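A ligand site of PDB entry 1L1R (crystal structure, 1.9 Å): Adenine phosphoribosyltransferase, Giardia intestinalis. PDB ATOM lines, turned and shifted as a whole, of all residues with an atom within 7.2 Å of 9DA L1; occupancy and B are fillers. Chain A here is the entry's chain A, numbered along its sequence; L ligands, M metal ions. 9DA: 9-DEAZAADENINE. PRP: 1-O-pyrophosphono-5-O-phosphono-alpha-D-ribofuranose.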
ATOM      1  N   ILE A  15       0.145 -10.600  14.421  1.00  0.00           N
ATOM      2  CA  ILE A  15       0.490 -10.381  13.018  1.00  0.00           C
ATOM      3  C   ILE A  15       1.906  -9.828  12.937  1.00  0.00           C
ATOM      4  O   ILE A  15       2.180  -8.736  13.408  1.00  0.00           O
ATOM      5  CB  ILE A  15      -0.463  -9.367  12.366  1.00  0.00           C
ATOM      6  CG1 ILE A  15      -1.923  -9.758  12.653  1.00  0.00           C
ATOM      7  CG2 ILE A  15      -0.203  -9.297  10.871  1.00  0.00           C
ATOM      8  CD1 ILE A  15      -2.322 -11.098  12.076  1.00  0.00           C
ATOM      9  N   PHE A  18       3.872  -5.685  11.223  1.00  0.00           N
ATOM     10  CA  PHE A  18       2.768  -4.763  11.037  1.00  0.00           C
ATOM     11  C   PHE A  18       2.711  -3.709  12.141  1.00  0.00           C
ATOM     12  O   PHE A  18       2.900  -4.036  13.312  1.00  0.00           O
ATOM     13  CB  PHE A  18       1.427  -5.506  11.006  1.00  0.00           C
ATOM     14  CG  PHE A  18       0.274  -4.614  10.637  1.00  0.00           C
ATOM     15  CD1 PHE A  18       0.009  -4.317   9.304  1.00  0.00           C
ATOM     16  CD2 PHE A  18      -0.505  -4.012  11.626  1.00  0.00           C
ATOM     17  CE1 PHE A  18      -1.014  -3.430   8.955  1.00  0.00           C
ATOM     18  CE2 PHE A  18      -1.521  -3.130  11.282  1.00  0.00           C
ATOM     19  CZ  PHE A  18      -1.771  -2.833   9.947  1.00  0.00           C
ATOM     20  N   PRO A  19       2.445  -2.442  11.784  1.00  0.00           N
ATOM     21  CA  PRO A  19       2.180  -1.887  10.447  1.00  0.00           C
ATOM     22  C   PRO A  19       3.430  -1.799   9.550  1.00  0.00           C
ATOM     23  O   PRO A  19       3.342  -1.417   8.377  1.00  0.00           O
ATOM     24  CB  PRO A  19       1.583  -0.525  10.748  1.00  0.00           C
ATOM     25  CG  PRO A  19       2.326  -0.121  11.981  1.00  0.00           C
ATOM     26  CD  PRO A  19       2.317  -1.386  12.815  1.00  0.00           C
ATOM     27  N   ILE A  23       7.773  -4.765  13.879  1.00  0.00           N
ATOM     28  CA  ILE A  23       6.765  -4.670  14.928  1.00  0.00           C
ATOM     29  C   ILE A  23       5.768  -5.833  14.833  1.00  0.00           C
ATOM     30  O   ILE A  23       5.137  -6.046  13.795  1.00  0.00           O
ATOM     31  CB  ILE A  23       5.960  -3.341  14.831  1.00  0.00           C
ATOM     32  CG1 ILE A  23       6.864  -2.150  15.182  1.00  0.00           C
ATOM     33  CG2 ILE A  23       4.750  -3.396  15.760  1.00  0.00           C
ATOM     34  CD1 ILE A  23       7.912  -1.813  14.129  1.00  0.00           C
ATOM     35  N   ALA A  24       5.644  -6.592  15.916  1.00  0.00           N
ATOM     36  CA  ALA A  24       4.707  -7.707  15.961  1.00  0.00           C
ATOM     37  C   ALA A  24       3.388  -7.168  16.521  1.00  0.00           C
ATOM     38  O   ALA A  24       3.233  -7.024  17.744  1.00  0.00           O
ATOM     39  CB  ALA A  24       5.248  -8.805  16.844  1.00  0.00           C
ATOM     40  N   PHE A  25       2.446  -6.878  15.638  1.00  0.00           N
ATOM     41  CA  PHE A  25       1.152  -6.330  16.021  1.00  0.00           C
ATOM     42  C   PHE A  25       0.247  -7.334  16.732  1.00  0.00           C
ATOM     43  O   PHE A  25       0.044  -8.453  16.269  1.00  0.00           O
ATOM     44  CB  PHE A  25       0.435  -5.794  14.789  1.00  0.00           C
ATOM     45  CG  PHE A  25      -0.702  -4.863  15.084  1.00  0.00           C
ATOM     46  CD1 PHE A  25      -0.462  -3.503  15.300  1.00  0.00           C
ATOM     47  CD2 PHE A  25      -2.009  -5.333  15.158  1.00  0.00           C
ATOM     48  CE1 PHE A  25      -1.518  -2.622  15.566  1.00  0.00           C
ATOM     49  CE2 PHE A  25      -3.080  -4.460  15.418  1.00  0.00           C
ATOM     50  CZ  PHE A  25      -2.834  -3.096  15.629  1.00  0.00           C
ATOM     51  N   LYS A  26      -0.285  -6.924  17.882  1.00  0.00           N
ATOM     52  CA  LYS A  26      -1.193  -7.742  18.650  1.00  0.00           C
ATOM     53  C   LYS A  26      -2.602  -7.266  18.262  1.00  0.00           C
ATOM     54  O   LYS A  26      -3.027  -6.183  18.651  1.00  0.00           O
ATOM     55  CB  LYS A  26      -0.952  -7.531  20.153  1.00  0.00           C
ATOM     56  CG  LYS A  26       0.345  -8.129  20.662  1.00  0.00           C
ATOM     57  CD  LYS A  26       0.277  -9.649  20.692  1.00  0.00           C
ATOM     58  CE  LYS A  26       1.586 -10.270  21.181  1.00  0.00           C
ATOM     59  NZ  LYS A  26       1.470 -11.751  21.346  1.00  0.00           N
ATOM     60  N   ASP A  27      -3.288  -8.082  17.466  1.00  0.00           N
ATOM     61  CA  ASP A  27      -4.627  -7.766  16.981  1.00  0.00           C
ATOM     62  C   ASP A  27      -5.702  -8.270  17.959  1.00  0.00           C
ATOM     63  O   ASP A  27      -5.921  -9.463  18.080  1.00  0.00           O
ATOM     64  CB  ASP A  27      -4.803  -8.406  15.593  1.00  0.00           C
ATOM     65  CG  ASP A  27      -6.157  -8.125  14.974  1.00  0.00           C
ATOM     66  OD1 ASP A  27      -6.808  -7.151  15.405  1.00  0.00           O
ATOM     67  OD2 ASP A  27      -6.562  -8.866  14.058  1.00  0.00           O
ATOM     68  N   LEU A  28      -6.368  -7.350  18.655  1.00  0.00           N
ATOM     69  CA  LEU A  28      -7.383  -7.750  19.638  1.00  0.00           C
ATOM     70  C   LEU A  28      -8.785  -7.738  19.044  1.00  0.00           C
ATOM     71  O   LEU A  28      -9.760  -7.933  19.743  1.00  0.00           O
ATOM     72  CB  LEU A  28      -7.377  -6.775  20.818  1.00  0.00           C
ATOM     73  CG  LEU A  28      -6.058  -6.328  21.440  1.00  0.00           C
ATOM     74  CD1 LEU A  28      -6.362  -5.509  22.685  1.00  0.00           C
ATOM     75  CD2 LEU A  28      -5.222  -7.523  21.785  1.00  0.00           C
ATOM     76  N   ARG A  63      -8.507   3.393  19.222  1.00  0.00           N
ATOM     77  CA  ARG A  63      -8.922   2.092  19.736  1.00  0.00           C
ATOM     78  C   ARG A  63      -9.382   2.153  21.190  1.00  0.00           C
ATOM     79  O   ARG A  63     -10.117   1.283  21.658  1.00  0.00           O
ATOM     80  CB  ARG A  63      -7.806   1.075  19.538  1.00  0.00           C
ATOM     81  CG  ARG A  63      -7.728   0.602  18.080  1.00  0.00           C
ATOM     82  CD  ARG A  63      -6.314   0.544  17.559  1.00  0.00           C
ATOM     83  NE  ARG A  63      -5.494  -0.362  18.335  1.00  0.00           N
ATOM     84  CZ  ARG A  63      -4.198  -0.567  18.133  1.00  0.00           C
ATOM     85  NH1 ARG A  63      -3.559   0.082  17.163  1.00  0.00           N
ATOM     86  NH2 ARG A  63      -3.540  -1.430  18.911  1.00  0.00           N
ATOM     87  N   MET A  99       5.166   7.278  20.276  1.00  0.00           N
ATOM     88  CA  MET A  99       4.779   5.908  20.615  1.00  0.00           C
ATOM     89  C   MET A  99       5.562   4.890  19.767  1.00  0.00           C
ATOM     90  O   MET A  99       6.379   5.272  18.933  1.00  0.00           O
ATOM     91  CB  MET A  99       3.260   5.699  20.499  1.00  0.00           C
ATOM     92  CG  MET A  99       2.594   6.204  19.220  1.00  0.00           C
ATOM     93  SD  MET A  99       2.736   5.059  17.811  1.00  0.00           S
ATOM     94  CE  MET A  99       1.866   3.626  18.431  1.00  0.00           C
ATOM     95  N   GLU A 100       5.314   3.591  19.979  1.00  0.00           N
ATOM     96  CA  GLU A 100       6.046   2.530  19.273  1.00  0.00           C
ATOM     97  C   GLU A 100       6.314   2.671  17.770  1.00  0.00           C
ATOM     98  O   GLU A 100       7.416   2.366  17.315  1.00  0.00           O
ATOM     99  CB  GLU A 100       5.401   1.161  19.519  1.00  0.00           C
ATOM    100  CG  GLU A 100       6.350  -0.004  19.191  1.00  0.00           C
ATOM    101  CD  GLU A 100       5.652  -1.352  19.141  1.00  0.00           C
ATOM    102  OE1 GLU A 100       4.738  -1.512  18.305  1.00  0.00           O
ATOM    103  OE2 GLU A 100       6.017  -2.250  19.925  1.00  0.00           O
ATOM    104  N   TYR A 101       5.324   3.116  16.987  1.00  0.00           N
ATOM    105  CA  TYR A 101       5.556   3.263  15.545  1.00  0.00           C
ATOM    106  C   TYR A 101       5.191   4.611  14.919  1.00  0.00           C
ATOM    107  O   TYR A 101       4.714   4.677  13.781  1.00  0.00           O
ATOM    108  CB  TYR A 101       4.864   2.109  14.789  1.00  0.00           C
ATOM    109  CG  TYR A 101       3.450   1.784  15.214  1.00  0.00           C
ATOM    110  CD1 TYR A 101       2.405   2.677  14.990  1.00  0.00           C
ATOM    111  CD2 TYR A 101       3.147   0.565  15.820  1.00  0.00           C
ATOM    112  CE1 TYR A 101       1.084   2.360  15.359  1.00  0.00           C
ATOM    113  CE2 TYR A 101       1.832   0.235  16.187  1.00  0.00           C
ATOM    114  CZ  TYR A 101       0.815   1.137  15.950  1.00  0.00           C
ATOM    115  OH  TYR A 101      -0.478   0.818  16.315  1.00  0.00           O
ATOM    116  N   ASP A 125      -6.540   0.613  24.763  1.00  0.00           N
ATOM    117  CA  ASP A 125      -6.532  -0.817  24.487  1.00  0.00           C
ATOM    118  C   ASP A 125      -5.220  -1.559  24.771  1.00  0.00           C
ATOM    119  O   ASP A 125      -5.232  -2.616  25.390  1.00  0.00           O
ATOM    120  CB  ASP A 125      -6.953  -1.090  23.040  1.00  0.00           C
ATOM    121  CG  ASP A 125      -5.987  -0.519  22.025  1.00  0.00           C
ATOM    122  OD1 ASP A 125      -5.903  -1.100  20.915  1.00  0.00           O
ATOM    123  OD2 ASP A 125      -5.322   0.495  22.311  1.00  0.00           O
ATOM    124  N   VAL A 126      -4.097  -0.995  24.344  1.00  0.00           N
ATOM    125  CA  VAL A 126      -2.809  -1.632  24.515  1.00  0.00           C
ATOM    126  C   VAL A 126      -1.745  -0.735  25.170  1.00  0.00           C
ATOM    127  O   VAL A 126      -1.600   0.443  24.817  1.00  0.00           O
ATOM    128  CB  VAL A 126      -2.232  -2.080  23.132  1.00  0.00           C
ATOM    129  CG1 VAL A 126      -0.805  -2.603  23.300  1.00  0.00           C
ATOM    130  CG2 VAL A 126      -3.105  -3.144  22.517  1.00  0.00           C
ATOM    131  N   LEU A 127      -1.023  -1.303  26.132  1.00  0.00           N
ATOM    132  CA  LEU A 127       0.064  -0.579  26.776  1.00  0.00           C
ATOM    133  C   LEU A 127       1.341  -1.160  26.178  1.00  0.00           C
ATOM    134  O   LEU A 127       1.675  -2.329  26.416  1.00  0.00           O
ATOM    135  CB  LEU A 127       0.066  -0.803  28.299  1.00  0.00           C
ATOM    136  CG  LEU A 127       1.329  -0.411  29.080  1.00  0.00           C
ATOM    137  CD1 LEU A 127       1.702   1.035  28.793  1.00  0.00           C
ATOM    138  CD2 LEU A 127       1.102  -0.618  30.582  1.00  0.00           C
ATOM    139  N   ALA A 128       2.022  -0.369  25.362  1.00  0.00           N
ATOM    140  CA  ALA A 128       3.281  -0.798  24.751  1.00  0.00           C
ATOM    141  C   ALA A 128       4.395  -0.114  25.523  1.00  0.00           C
ATOM    142  O   ALA A 128       4.704  -0.516  26.643  1.00  0.00           O
ATOM    143  CB  ALA A 128       3.325  -0.402  23.279  1.00  0.00           C
ATOM    144  N   THR A 129       4.961   0.942  24.956  1.00  0.00           N
ATOM    145  CA  THR A 129       6.036   1.674  25.625  1.00  0.00           C
ATOM    146  C   THR A 129       5.504   2.483  26.801  1.00  0.00           C
ATOM    147  O   THR A 129       6.154   2.584  27.848  1.00  0.00           O
ATOM    148  CB  THR A 129       6.735   2.668  24.662  1.00  0.00           C
ATOM    149  OG1 THR A 129       5.842   3.741  24.350  1.00  0.00           O
ATOM    150  CG2 THR A 129       7.137   1.963  23.371  1.00  0.00           C
ATOM    151  N   TYR A 156      -4.844  -4.849  27.059  1.00  0.00           N
ATOM    152  CA  TYR A 156      -3.672  -5.701  26.870  1.00  0.00           C
ATOM    153  C   TYR A 156      -2.359  -5.012  27.249  1.00  0.00           C
ATOM    154  O   TYR A 156      -2.078  -3.911  26.796  1.00  0.00           O
ATOM    155  CB  TYR A 156      -3.637  -6.106  25.396  1.00  0.00           C
ATOM    156  CG  TYR A 156      -2.644  -7.173  25.052  1.00  0.00           C
ATOM    157  CD1 TYR A 156      -2.898  -8.510  25.362  1.00  0.00           C
ATOM    158  CD2 TYR A 156      -1.463  -6.873  24.384  1.00  0.00           C
ATOM    159  CE1 TYR A 156      -2.011  -9.520  25.009  1.00  0.00           C
ATOM    160  CE2 TYR A 156      -0.563  -7.867  24.024  1.00  0.00           C
ATOM    161  CZ  TYR A 156      -0.837  -9.190  24.337  1.00  0.00           C
ATOM    162  OH  TYR A 156       0.060 -10.181  24.007  1.00  0.00           O
ATOM    163  N   ILE A 158       1.782  -5.305  27.121  1.00  0.00           N
ATOM    164  CA  ILE A 158       2.972  -5.956  26.592  1.00  0.00           C
ATOM    165  C   ILE A 158       4.099  -5.710  27.596  1.00  0.00           C
ATOM    166  O   ILE A 158       4.877  -4.771  27.441  1.00  0.00           O
ATOM    167  CB  ILE A 158       3.354  -5.369  25.234  1.00  0.00           C
ATOM    168  CG1 ILE A 158       2.196  -5.571  24.260  1.00  0.00           C
ATOM    169  CG2 ILE A 158       4.623  -6.036  24.713  1.00  0.00           C
ATOM    170  CD1 ILE A 158       2.334  -4.807  22.972  1.00  0.00           C
ATOM    171  N   LEU A 161       8.070  -4.376  26.865  1.00  0.00           N
ATOM    172  CA  LEU A 161       8.552  -3.004  26.753  1.00  0.00           C
ATOM    173  C   LEU A 161       8.474  -2.200  28.050  1.00  0.00           C
ATOM    174  O   LEU A 161       8.706  -1.004  28.037  1.00  0.00           O
ATOM    175  CB  LEU A 161       7.757  -2.276  25.663  1.00  0.00           C
ATOM    176  CG  LEU A 161       7.543  -3.049  24.353  1.00  0.00           C
ATOM    177  CD1 LEU A 161       6.722  -2.212  23.387  1.00  0.00           C
ATOM    178  CD2 LEU A 161       8.883  -3.403  23.748  1.00  0.00           C
ATOM    179  N   GLU A 180       0.686 -10.019  28.153  1.00  0.00           N
ATOM    180  CA  GLU A 180       1.241 -10.907  27.138  1.00  0.00           C
ATOM    181  C   GLU A 180       2.010 -12.065  27.772  1.00  0.00           C
ATOM    182  O   GLU A 180       2.669 -11.837  28.801  1.00  0.00           O
ATOM    183  CB  GLU A 180       2.150 -10.126  26.205  1.00  0.00           C
ATOM    184  CG  GLU A 180       2.776 -10.975  25.115  1.00  0.00           C
ATOM    185  CD  GLU A 180       3.521 -10.143  24.092  1.00  0.00           C
ATOM    186  OE1 GLU A 180       4.155 -10.729  23.201  1.00  0.00           O
ATOM    187  OE2 GLU A 180       3.468  -8.903  24.193  1.00  0.00           O
HETATM  188  N1  9DA L   1       0.244  -4.295  18.927  1.00  0.00           N
HETATM  189  C2  9DA L   1      -0.967  -3.612  18.930  1.00  0.00           C
HETATM  190  N3  9DA L   1      -1.034  -2.296  19.148  1.00  0.00           N
HETATM  191  C4  9DA L   1       0.193  -1.714  19.351  1.00  0.00           C
HETATM  192  C5  9DA L   1       1.435  -2.333  19.359  1.00  0.00           C
HETATM  193  C6  9DA L   1       1.526  -3.739  19.122  1.00  0.00           C
HETATM  194  N6  9DA L   1       2.519  -4.486  19.086  1.00  0.00           N
HETATM  195  N7  9DA L   1       2.400  -1.372  19.604  1.00  0.00           N
HETATM  196  C8  9DA L   1       1.751  -0.195  19.743  1.00  0.00           C
HETATM  197  C9  9DA L   1       0.386  -0.358  19.596  1.00  0.00           C
HETATM  198  C1  PRP L   2      -1.592   2.429  19.662  1.00  0.00           C
HETATM  199  C2  PRP L   2      -2.390   1.697  20.760  1.00  0.00           C
HETATM  200  C3  PRP L   2      -2.061   2.490  22.012  1.00  0.00           C
HETATM  201  C4  PRP L   2      -0.660   2.977  21.807  1.00  0.00           C
HETATM  202  C5  PRP L   2       0.242   2.219  22.512  1.00  0.00           C
HETATM  203  O1  PRP L   2      -2.455   3.490  19.166  1.00  0.00           O
HETATM  204  O2  PRP L   2      -3.779   1.688  20.420  1.00  0.00           O
HETATM  205  O3  PRP L   2      -2.986   3.604  22.107  1.00  0.00           O
HETATM  206  O4  PRP L   2      -0.446   2.918  20.321  1.00  0.00           O
HETATM  207  O5  PRP L   2       1.611   2.525  22.266  1.00  0.00           O
HETATM  208  P   PRP L   2       2.590   3.131  23.386  1.00  0.00           P
HETATM  209  O1P PRP L   2       2.390   2.372  24.692  1.00  0.00           O
HETATM  210  O2P PRP L   2       2.331   4.631  23.495  1.00  0.00           O
HETATM  211  O3P PRP L   2       3.959   2.800  22.780  1.00  0.00           O
HETATM  212  PA  PRP L   2      -2.143   4.261  17.779  1.00  0.00           P
HETATM  213  O1A PRP L   2      -1.233   5.390  18.062  1.00  0.00           O
HETATM  214  O2A PRP L   2      -1.661   3.252  16.783  1.00  0.00           O
HETATM  215  O3A PRP L   2      -3.596   4.847  17.419  1.00  0.00           O
HETATM  216  PB  PRP L   2      -4.991   4.076  17.027  1.00  0.00           P
HETATM  217  O1B PRP L   2      -4.578   2.773  16.319  1.00  0.00           O
HETATM  218  O2B PRP L   2      -5.776   5.034  16.163  1.00  0.00           O
HETATM  219  O3B PRP L   2      -5.676   3.800  18.324  1.00  0.00           O
HETATM  220 MG    MG M   1      -4.428   4.132  20.162  1.00  0.00          MG
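Merely in contact with 9DA L1: Phe 25 (3.5 Å), Tyr 101 (3.6 Å), Ala 128 (3.9 Å) and Ile 158 (3.9 Å).
Hydrophobic or aromatic side chains that line 9DA L1: Phe 25, Tyr 101, Ala 128 and Ile 158.
Within 4 Å of 9DA L1: Ala 24, Phe 25, Lys 26, Arg 63, Glu 100, Tyr 101, Ala 128 and Ile 158.
NZ of Lys 26 lies close to OH of Tyr 156, 3.4 Å away.
SD of Met 99 sits close to N of Tyr 101 (3.3 Å).
The side-chain hydroxyl (OH) of Tyr 101 lies within hydrogen-bond range of the guanidinium group (NH1) of Arg 63 (3.3 Å).
The guanidinium group (NE) of Arg 63 is in salt-bridge range of the side-chain carboxylate (OD1) of Asp 125.
The side-chain carboxylate (OE1) of Glu 180 lies within salt-bridge range of the side-chain amino group (NZ) of Lys 26 (3.4 Å).
The backbone NH (N) of Ile 158 is in hydrogen-bond range of the backbone carbonyl oxygen (O) of Leu 127 (3.1 Å).
The backbone carbonyl oxygen (O) of Phe 25 sits at hydrogen-bond distance from the backbone NH (N) of Ile 15, at 2.8 Å.
An oxygen (O2A) of PRP L2 sits at hydrogen-bond distance from the side-chain hydroxyl (OH) of Tyr 101 (2.7 Å).
A nitrogen (N7) of 9DA L1 is in hydrogen-bond range of the side-chain carboxylate (OE1) of Glu 100, 2.7 Å away.
O1P of PRP L2 lies within hydrogen-bond range of N of Thr 129 (3.0 Å).
The guanidinium group (NH2) of Arg 63 lies within hydrogen-bond range of a nitrogen (N3) of 9DA L1, 2.7 Å away.
An oxygen (O1B) of PRP L2 is in salt-bridge range of the guanidinium group (NH1) of Arg 63 (3.0 Å).
The side-chain hydroxyl (OG1) of Thr 129 sits at hydrogen-bond distance from an oxygen (O3P) of PRP L2, at 2.6 Å.
N of Glu 100 lies within hydrogen-bond range of O3P of PRP L2 (3.2 Å).
An oxygen (O2) of PRP L2 lies close to the side-chain carboxylate (OD2) of Asp 125 (2.7 Å).
The backbone NH (N) of Lys 26 is in hydrogen-bond range of a nitrogen (N1) of 9DA L1 (2.9 Å).
The backbone NH (N) of Ala 128 lies within hydrogen-bond range of an oxygen (O1P) of PRP L2 (2.8 Å).
O of Ala 24 sits at hydrogen-bond distance from N6 of 9DA L1 (3.0 Å).
An oxygen (O3B) of PRP L2 lies close to the backbone NH (N) of Arg 63, at 3.0 Å.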
